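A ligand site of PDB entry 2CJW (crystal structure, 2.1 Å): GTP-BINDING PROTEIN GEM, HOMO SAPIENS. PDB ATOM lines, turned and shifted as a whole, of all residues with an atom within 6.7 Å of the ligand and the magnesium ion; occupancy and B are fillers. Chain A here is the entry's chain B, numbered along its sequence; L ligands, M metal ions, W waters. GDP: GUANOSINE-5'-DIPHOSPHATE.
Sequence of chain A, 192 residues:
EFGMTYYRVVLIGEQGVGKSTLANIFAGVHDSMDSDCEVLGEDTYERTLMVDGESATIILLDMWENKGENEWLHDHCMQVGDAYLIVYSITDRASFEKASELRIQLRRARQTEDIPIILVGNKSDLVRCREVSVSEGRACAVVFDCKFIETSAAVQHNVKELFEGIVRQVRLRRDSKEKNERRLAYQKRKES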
ATOM      1  N   GLY A  13      16.353  -2.724  27.245  1.00  0.00           N
ATOM      2  CA  GLY A  13      17.683  -2.646  27.806  1.00  0.00           C
ATOM      3  C   GLY A  13      17.836  -1.373  28.620  1.00  0.00           C
ATOM      4  O   GLY A  13      16.917  -0.547  28.661  1.00  0.00           O
ATOM      5  N   GLU A  14      18.992  -1.229  29.257  1.00  0.00           N
ATOM      6  CA  GLU A  14      19.234  -0.120  30.181  1.00  0.00           C
ATOM      7  C   GLU A  14      19.347   1.208  29.458  1.00  0.00           C
ATOM      8  O   GLU A  14      19.738   1.256  28.292  1.00  0.00           O
ATOM      9  CB  GLU A  14      20.505  -0.377  31.006  1.00  0.00           C
ATOM     10  CG  GLU A  14      20.325  -1.384  32.140  1.00  0.00           C
ATOM     11  CD  GLU A  14      19.278  -0.934  33.155  1.00  0.00           C
ATOM     12  OE1 GLU A  14      18.258  -1.645  33.303  1.00  0.00           O
ATOM     13  OE2 GLU A  14      19.453   0.123  33.785  1.00  0.00           O
ATOM     14  N   GLN A  15      19.012   2.283  30.156  1.00  0.00           N
ATOM     15  CA  GLN A  15      19.205   3.624  29.627  1.00  0.00           C
ATOM     16  C   GLN A  15      20.663   3.829  29.212  1.00  0.00           C
ATOM     17  O   GLN A  15      21.580   3.437  29.932  1.00  0.00           O
ATOM     18  CB  GLN A  15      18.797   4.666  30.675  1.00  0.00           C
ATOM     19  CG  GLN A  15      18.588   6.067  30.109  1.00  0.00           C
ATOM     20  CD  GLN A  15      18.294   7.097  31.193  1.00  0.00           C
ATOM     21  OE1 GLN A  15      17.653   6.793  32.207  1.00  0.00           O
ATOM     22  NE2 GLN A  15      18.739   8.338  30.967  1.00  0.00           N
ATOM     23  N   GLY A  16      20.864   4.409  28.035  1.00  0.00           N
ATOM     24  CA  GLY A  16      22.191   4.779  27.566  1.00  0.00           C
ATOM     25  C   GLY A  16      22.966   3.739  26.792  1.00  0.00           C
ATOM     26  O   GLY A  16      24.121   3.976  26.405  1.00  0.00           O
ATOM     27  N   VAL A  17      22.350   2.581  26.546  1.00  0.00           N
ATOM     28  CA  VAL A  17      23.020   1.508  25.808  1.00  0.00           C
ATOM     29  C   VAL A  17      23.060   1.749  24.289  1.00  0.00           C
ATOM     30  O   VAL A  17      23.958   1.267  23.599  1.00  0.00           O
ATOM     31  CB  VAL A  17      22.441   0.089  26.130  1.00  0.00           C
ATOM     32  CG1 VAL A  17      22.653  -0.265  27.596  1.00  0.00           C
ATOM     33  CG2 VAL A  17      20.969  -0.020  25.736  1.00  0.00           C
ATOM     34  N   GLY A  18      22.080   2.502  23.782  1.00  0.00           N
ATOM     35  CA  GLY A  18      22.048   2.894  22.365  1.00  0.00           C
ATOM     36  C   GLY A  18      20.804   2.443  21.618  1.00  0.00           C
ATOM     37  O   GLY A  18      20.837   2.343  20.392  1.00  0.00           O
ATOM     38  N   LYS A  19      19.729   2.190  22.350  1.00  0.00           N
ATOM     39  CA  LYS A  19      18.471   1.703  21.780  1.00  0.00           C
ATOM     40  C   LYS A  19      17.919   2.681  20.726  1.00  0.00           C
ATOM     41  O   LYS A  19      17.556   2.273  19.629  1.00  0.00           O
ATOM     42  CB  LYS A  19      17.431   1.458  22.870  1.00  0.00           C
ATOM     43  CG  LYS A  19      17.819   0.362  23.879  1.00  0.00           C
ATOM     44  CD  LYS A  19      16.672   0.017  24.839  1.00  0.00           C
ATOM     45  CE  LYS A  19      16.258   1.188  25.754  1.00  0.00           C
ATOM     46  NZ  LYS A  19      17.394   1.856  26.426  1.00  0.00           N
ATOM     47  N   SER A  20      17.889   3.951  21.094  1.00  0.00           N
ATOM     48  CA  SER A  20      17.382   5.020  20.220  1.00  0.00           C
ATOM     49  C   SER A  20      18.279   5.296  19.029  1.00  0.00           C
ATOM     50  O   SER A  20      17.788   5.627  17.956  1.00  0.00           O
ATOM     51  CB  SER A  20      17.165   6.298  21.031  1.00  0.00           C
ATOM     52  OG  SER A  20      16.132   6.093  21.973  1.00  0.00           O
ATOM     53  N   THR A  21      19.592   5.183  19.233  1.00  0.00           N
ATOM     54  CA  THR A  21      20.566   5.408  18.172  1.00  0.00           C
ATOM     55  C   THR A  21      20.471   4.300  17.115  1.00  0.00           C
ATOM     56  O   THR A  21      20.600   4.555  15.913  1.00  0.00           O
ATOM     57  CB  THR A  21      22.012   5.515  18.740  1.00  0.00           C
ATOM     58  OG1 THR A  21      22.041   6.499  19.798  1.00  0.00           O
ATOM     59  CG2 THR A  21      22.994   5.944  17.665  1.00  0.00           C
ATOM     60  N   LEU A  22      20.227   3.071  17.577  1.00  0.00           N
ATOM     61  CA  LEU A  22      19.943   1.962  16.685  1.00  0.00           C
ATOM     62  C   LEU A  22      18.631   2.180  15.928  1.00  0.00           C
ATOM     63  O   LEU A  22      18.553   1.958  14.712  1.00  0.00           O
ATOM     64  CB  LEU A  22      19.903   0.639  17.468  1.00  0.00           C
ATOM     65  CG  LEU A  22      21.269   0.091  17.929  1.00  0.00           C
ATOM     66  CD1 LEU A  22      21.087  -1.026  18.950  1.00  0.00           C
ATOM     67  CD2 LEU A  22      22.079  -0.415  16.759  1.00  0.00           C
ATOM     68  N   ASN A  24      17.280   5.029  15.243  1.00  0.00           N
ATOM     69  CA  ASN A  24      17.567   6.096  14.293  1.00  0.00           C
ATOM     70  C   ASN A  24      18.239   5.633  13.001  1.00  0.00           C
ATOM     71  O   ASN A  24      17.912   6.123  11.919  1.00  0.00           O
ATOM     72  CB  ASN A  24      18.377   7.193  14.947  1.00  0.00           C
ATOM     73  CG  ASN A  24      17.497   8.229  15.606  1.00  0.00           C
ATOM     74  OD1 ASN A  24      17.090   9.192  14.968  1.00  0.00           O
ATOM     75  ND2 ASN A  24      17.174   8.006  16.875  1.00  0.00           N
ATOM     76  N   ASP A  62      10.509   1.637  20.360  1.00  0.00           N
ATOM     77  CA  ASP A  62      11.608   2.137  21.183  1.00  0.00           C
ATOM     78  C   ASP A  62      11.006   2.987  22.299  1.00  0.00           C
ATOM     79  O   ASP A  62      11.096   4.210  22.286  1.00  0.00           O
ATOM     80  CB  ASP A  62      12.578   2.954  20.326  1.00  0.00           C
ATOM     81  CG  ASP A  62      13.702   3.619  21.150  1.00  0.00           C
ATOM     82  OD1 ASP A  62      14.263   2.985  22.061  1.00  0.00           O
ATOM     83  OD2 ASP A  62      14.020   4.795  20.860  1.00  0.00           O
ATOM     84  N   TRP A  64      10.966   1.553  25.800  1.00  0.00           N
ATOM     85  CA  TRP A  64      11.274   0.840  27.041  1.00  0.00           C
ATOM     86  C   TRP A  64      11.766   1.781  28.124  1.00  0.00           C
ATOM     87  O   TRP A  64      12.699   2.559  27.901  1.00  0.00           O
ATOM     88  CB  TRP A  64      12.296  -0.261  26.790  1.00  0.00           C
ATOM     89  CG  TRP A  64      12.710  -1.014  28.032  1.00  0.00           C
ATOM     90  CD1 TRP A  64      13.830  -0.797  28.786  1.00  0.00           C
ATOM     91  CD2 TRP A  64      12.005  -2.107  28.639  1.00  0.00           C
ATOM     92  NE1 TRP A  64      13.867  -1.695  29.827  1.00  0.00           N
ATOM     93  CE2 TRP A  64      12.757  -2.502  29.764  1.00  0.00           C
ATOM     94  CE3 TRP A  64      10.818  -2.774  28.352  1.00  0.00           C
ATOM     95  CZ2 TRP A  64      12.366  -3.549  30.603  1.00  0.00           C
ATOM     96  CZ3 TRP A  64      10.421  -3.823  29.182  1.00  0.00           C
ATOM     97  CH2 TRP A  64      11.194  -4.199  30.285  1.00  0.00           C
ATOM     98  N   VAL A  87      19.486  -4.993  24.338  1.00  0.00           N
ATOM     99  CA  VAL A  87      20.719  -4.271  24.057  1.00  0.00           C
ATOM    100  C   VAL A  87      21.450  -3.970  25.362  1.00  0.00           C
ATOM    101  O   VAL A  87      20.839  -3.530  26.347  1.00  0.00           O
ATOM    102  CB  VAL A  87      20.438  -2.933  23.284  1.00  0.00           C
ATOM    103  CG1 VAL A  87      21.749  -2.284  22.831  1.00  0.00           C
ATOM    104  CG2 VAL A  87      19.519  -3.160  22.090  1.00  0.00           C
ATOM    105  N   ASN A 122      26.202  -3.530  21.893  1.00  0.00           N
ATOM    106  CA  ASN A 122      26.403  -2.252  21.189  1.00  0.00           C
ATOM    107  C   ASN A 122      27.659  -1.506  21.643  1.00  0.00           C
ATOM    108  O   ASN A 122      28.180  -1.767  22.734  1.00  0.00           O
ATOM    109  CB  ASN A 122      25.159  -1.369  21.330  1.00  0.00           C
ATOM    110  CG  ASN A 122      25.163  -0.179  20.350  1.00  0.00           C
ATOM    111  OD1 ASN A 122      25.521  -0.316  19.184  1.00  0.00           O
ATOM    112  ND2 ASN A 122      24.755   0.983  20.852  1.00  0.00           N
ATOM    113  N   LYS A 123      28.123  -0.573  20.804  1.00  0.00           N
ATOM    114  CA  LYS A 123      29.300   0.281  21.058  1.00  0.00           C
ATOM    115  C   LYS A 123      30.641  -0.429  20.822  1.00  0.00           C
ATOM    116  O   LYS A 123      31.663  -0.083  21.435  1.00  0.00           O
ATOM    117  CB  LYS A 123      29.259   0.963  22.443  1.00  0.00           C
ATOM    118  CG  LYS A 123      27.989   1.773  22.681  1.00  0.00           C
ATOM    119  CD  LYS A 123      28.002   2.575  23.983  1.00  0.00           C
ATOM    120  CE  LYS A 123      26.718   3.388  24.128  1.00  0.00           C
ATOM    121  NZ  LYS A 123      26.632   4.219  25.363  1.00  0.00           N
ATOM    122  N   SER A 124      30.635  -1.389  19.893  1.00  0.00           N
ATOM    123  CA  SER A 124      31.842  -2.149  19.528  1.00  0.00           C
ATOM    124  C   SER A 124      32.974  -1.294  18.926  1.00  0.00           C
ATOM    125  O   SER A 124      34.094  -1.786  18.761  1.00  0.00           O
ATOM    126  CB  SER A 124      31.483  -3.320  18.597  1.00  0.00           C
ATOM    127  OG  SER A 124      30.940  -2.866  17.363  1.00  0.00           O
ATOM    128  N   ASP A 125      32.681  -0.032  18.600  1.00  0.00           N
ATOM    129  CA  ASP A 125      33.705   0.913  18.148  1.00  0.00           C
ATOM    130  C   ASP A 125      34.638   1.374  19.273  1.00  0.00           C
ATOM    131  O   ASP A 125      35.796   1.712  19.029  1.00  0.00           O
ATOM    132  CB  ASP A 125      33.067   2.132  17.470  1.00  0.00           C
ATOM    133  CG  ASP A 125      32.063   2.832  18.366  1.00  0.00           C
ATOM    134  OD1 ASP A 125      30.992   2.235  18.639  1.00  0.00           O
ATOM    135  OD2 ASP A 125      32.324   3.981  18.797  1.00  0.00           O
ATOM    136  N   LEU A 126      34.120   1.376  20.501  1.00  0.00           N
ATOM    137  CA  LEU A 126      34.875   1.821  21.672  1.00  0.00           C
ATOM    138  C   LEU A 126      35.775   0.712  22.248  1.00  0.00           C
ATOM    139  O   LEU A 126      35.577   0.255  23.379  1.00  0.00           O
ATOM    140  CB  LEU A 126      33.919   2.357  22.758  1.00  0.00           C
ATOM    141  CG  LEU A 126      33.000   3.538  22.416  1.00  0.00           C
ATOM    142  CD1 LEU A 126      32.203   3.954  23.635  1.00  0.00           C
ATOM    143  CD2 LEU A 126      33.784   4.720  21.835  1.00  0.00           C
ATOM    144  N   THR A 151      27.245  -4.730  17.696  1.00  0.00           N
ATOM    145  CA  THR A 151      26.971  -3.640  16.761  1.00  0.00           C
ATOM    146  C   THR A 151      27.709  -2.382  17.165  1.00  0.00           C
ATOM    147  O   THR A 151      27.992  -2.155  18.346  1.00  0.00           O
ATOM    148  CB  THR A 151      25.476  -3.284  16.720  1.00  0.00           C
ATOM    149  OG1 THR A 151      25.066  -2.810  18.009  1.00  0.00           O
ATOM    150  CG2 THR A 151      24.616  -4.486  16.320  1.00  0.00           C
ATOM    151  N   SER A 152      27.998  -1.546  16.180  1.00  0.00           N
ATOM    152  CA  SER A 152      28.325  -0.149  16.448  1.00  0.00           C
ATOM    153  C   SER A 152      27.302   0.731  15.747  1.00  0.00           C
ATOM    154  O   SER A 152      27.206   0.739  14.514  1.00  0.00           O
ATOM    155  CB  SER A 152      29.740   0.195  16.002  1.00  0.00           C
ATOM    156  OG  SER A 152      29.975   1.576  16.228  1.00  0.00           O
ATOM    157  N   ALA A 153      26.529   1.451  16.557  1.00  0.00           N
ATOM    158  CA  ALA A 153      25.514   2.370  16.056  1.00  0.00           C
ATOM    159  C   ALA A 153      26.157   3.674  15.587  1.00  0.00           C
ATOM    160  O   ALA A 153      25.658   4.310  14.655  1.00  0.00           O
ATOM    161  CB  ALA A 153      24.466   2.633  17.126  1.00  0.00           C
ATOM    162  N   ALA A 154      27.250   4.073  16.219  1.00  0.00           N
ATOM    163  CA  ALA A 154      27.960   5.298  15.843  1.00  0.00           C
ATOM    164  C   ALA A 154      28.611   5.186  14.456  1.00  0.00           C
ATOM    165  O   ALA A 154      28.529   6.117  13.656  1.00  0.00           O
ATOM    166  CB  ALA A 154      28.994   5.670  16.889  1.00  0.00           C
ATOM    167  N   VAL A 155      29.229   4.040  14.180  1.00  0.00           N
ATOM    168  CA  VAL A 155      29.983   3.842  12.954  1.00  0.00           C
ATOM    169  C   VAL A 155      29.226   2.952  11.931  1.00  0.00           C
ATOM    170  O   VAL A 155      29.724   2.662  10.846  1.00  0.00           O
ATOM    171  CB  VAL A 155      31.419   3.303  13.271  1.00  0.00           C
ATOM    172  CG1 VAL A 155      32.301   3.204  12.019  1.00  0.00           C
ATOM    173  CG2 VAL A 155      32.103   4.194  14.296  1.00  0.00           C
ATOM    174  N   GLN A 156      27.995   2.556  12.286  1.00  0.00           N
ATOM    175  CA  GLN A 156      27.197   1.614  11.491  1.00  0.00           C
ATOM    176  C   GLN A 156      27.968   0.335  11.153  1.00  0.00           C
ATOM    177  O   GLN A 156      28.601   0.227  10.098  1.00  0.00           O
ATOM    178  CB  GLN A 156      26.658   2.263  10.198  1.00  0.00           C
ATOM    179  CG  GLN A 156      25.479   3.194  10.391  1.00  0.00           C
ATOM    180  CD  GLN A 156      24.885   3.646   9.067  1.00  0.00           C
ATOM    181  OE1 GLN A 156      25.193   4.735   8.569  1.00  0.00           O
ATOM    182  NE2 GLN A 156      24.038   2.801   8.478  1.00  0.00           N
HETATM  183  PB  GDP L   1      19.241   4.586  24.931  1.00  0.00           P
HETATM  184  O1B GDP L   1      18.876   5.227  26.257  1.00  0.00           O
HETATM  185  O2B GDP L   1      18.175   4.900  23.923  1.00  0.00           O
HETATM  186  O3B GDP L   1      19.341   3.089  25.120  1.00  0.00           O
HETATM  187  O3A GDP L   1      20.676   5.118  24.416  1.00  0.00           O
HETATM  188  PA  GDP L   1      20.864   6.288  23.321  1.00  0.00           P
HETATM  189  O1A GDP L   1      20.395   5.856  21.949  1.00  0.00           O
HETATM  190  O2A GDP L   1      20.151   7.547  23.753  1.00  0.00           O
HETATM  191  O5' GDP L   1      22.460   6.451  23.309  1.00  0.00           O
HETATM  192  C5' GDP L   1      23.159   6.963  24.459  1.00  0.00           C
HETATM  193  C4' GDP L   1      24.480   7.585  24.021  1.00  0.00           C
HETATM  194  O4' GDP L   1      25.338   6.540  23.548  1.00  0.00           O
HETATM  195  C3' GDP L   1      24.339   8.606  22.897  1.00  0.00           C
HETATM  196  O3' GDP L   1      25.029   9.800  23.244  1.00  0.00           O
HETATM  197  C2' GDP L   1      24.982   7.949  21.683  1.00  0.00           C
HETATM  198  O2' GDP L   1      25.746   8.864  20.864  1.00  0.00           O
HETATM  199  C1' GDP L   1      25.889   6.891  22.274  1.00  0.00           C
HETATM  200  N9  GDP L   1      25.943   5.680  21.429  1.00  0.00           N
HETATM  201  C8  GDP L   1      24.911   4.915  21.038  1.00  0.00           C
HETATM  202  N7  GDP L   1      25.336   3.882  20.272  1.00  0.00           N
HETATM  203  C5  GDP L   1      26.677   3.984  20.185  1.00  0.00           C
HETATM  204  C6  GDP L   1      27.763   3.225  19.521  1.00  0.00           C
HETATM  205  O6  GDP L   1      27.506   2.205  18.848  1.00  0.00           O
HETATM  206  N1  GDP L   1      29.027   3.664  19.666  1.00  0.00           N
HETATM  207  C2  GDP L   1      29.330   4.763  20.380  1.00  0.00           C
HETATM  208  N2  GDP L   1      30.631   5.151  20.478  1.00  0.00           N
HETATM  209  N3  GDP L   1      28.390   5.512  21.005  1.00  0.00           N
HETATM  210  C4  GDP L   1      27.077   5.165  20.941  1.00  0.00           C
HETATM  211 MG    MG M   1      16.426   6.176  24.215  1.00  0.00          MG
HETATM  212  O   HOH W   1      17.689   7.913  23.977  1.00  0.00           O
HETATM  213  O   HOH W   2      16.453   6.000  26.384  1.00  0.00           O
HETATM  214  O   HOH W   3      15.172   4.418  24.224  1.00  0.00           O
HETATM  215  O   HOH W   4      28.508   6.360  24.288  1.00  0.00           O
HETATM  216  O   HOH W   5      14.744   7.125  24.293  1.00  0.00           O
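The magnesium ion is bound by water W5 (1.9 Å), water W3 (2.2 Å), water W1 (2.2 Å), water W2 (2.2 Å), an oxygen (O2B) of the ligand (2.2 Å) and the side-chain hydroxyl of Ser 20 (2.3 Å).
The magnesium ion has six donor atoms within binding distance.
The nearest printed residue that does not touch the magnesium ion is Asp 62 (4.4 Å).
The side-chain hydroxyl (OG) of Ser 20 lies close to the side-chain carboxylate (OD2) of Asp 62, at 2.7 Å.
The backbone carbonyl oxygen (O) of Ser 20 lies within hydrogen-bond range of the side-chain amide nitrogen (ND2) of Asn 24 (2.7 Å).
The backbone NH (N) of Ala 153 is in hydrogen-bond range of the side-chain amide oxygen (OD1) of Asn 122 (3.3 Å).
The side-chain amino group of Lys 19 lies within hydrogen-bond range of the backbone carbonyl oxygen of Glu 14, at 3.1 Å.
The side-chain hydroxyl of Thr 151 is in hydrogen-bond range of the side-chain amide oxygen of Asn 122 (2.8 Å).
The backbone carbonyl oxygen of Thr 151 lies within hydrogen-bond range of the backbone NH of Lys 123 (2.9 Å).
The backbone NH of Ser 152 sits at hydrogen-bond distance from the side-chain hydroxyl of Ser 124.
N of Val 155 sits at hydrogen-bond distance from OG of Ser 152, at 3.3 Å.
Merely in contact with the ligand: Ser 152 (3.4 Å), Leu 126 (3.5 Å), Glu 14 (3.7 Å) and Gln 15 (3.7 Å).
Hydrophobic or aromatic side chains within 4 Å of the ligand: Val 17, Leu 126, Ala 153 and Ala 154.
Of the 25 residues printed, 15 come within 4 Å of the ligand.
Along chain A the residues within 4 Å of the ligand span positions 14 to 154.
The nearest printed residue that does not touch the ligand is Thr 151 (4.4 Å).
Water W4 lies within hydrogen-bond range of NZ of Lys 123 (3.0 Å) and O4' of the ligand (3.3 Å).
N of Ser 20 lies within hydrogen-bond range of O1A of the ligand, at 3.3 Å.
The backbone NH (N) of Ala 153 is in hydrogen-bond range of an oxygen (O6) of the ligand, at 2.6 Å.
N1 of the ligand is in hydrogen-bond range of OD1 of Asp 125, at 2.6 Å.
The backbone NH (N) of Lys 19 lies within hydrogen-bond range of an oxygen (O3B) of the ligand (2.9 Å).
NZ of Lys 19 lies within salt-bridge range of O3B of the ligand, 2.6 Å away.
The backbone NH of Thr 21 sits at hydrogen-bond distance from an oxygen (O1A) of the ligand (2.9 Å).
An oxygen (O1A) of the ligand lies within hydrogen-bond range of the side-chain hydroxyl (OG1) of Thr 21 (2.8 Å).
The backbone NH (N) of Gly 16 lies within hydrogen-bond range of an oxygen (O1B) of the ligand, 2.8 Å away.
The side-chain amide nitrogen (ND2) of Asn 122 sits at hydrogen-bond distance from a nitrogen (N7) of the ligand (3.0 Å).
N of Gly 18 is in hydrogen-bond range of O3A of the ligand (3.0 Å).
N of Lys 123 lies close to O6 of the ligand (3.5 Å).
The side-chain amino group (NZ) of Lys 123 lies within hydrogen-bond range of an oxygen (O4') of the ligand, 3.2 Å away.
The backbone NH of Ala 154 sits at hydrogen-bond distance from an oxygen (O6) of the ligand, at 3.2 Å.
O3B of the ligand sits at hydrogen-bond distance from N of Val 17 (3.4 Å).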
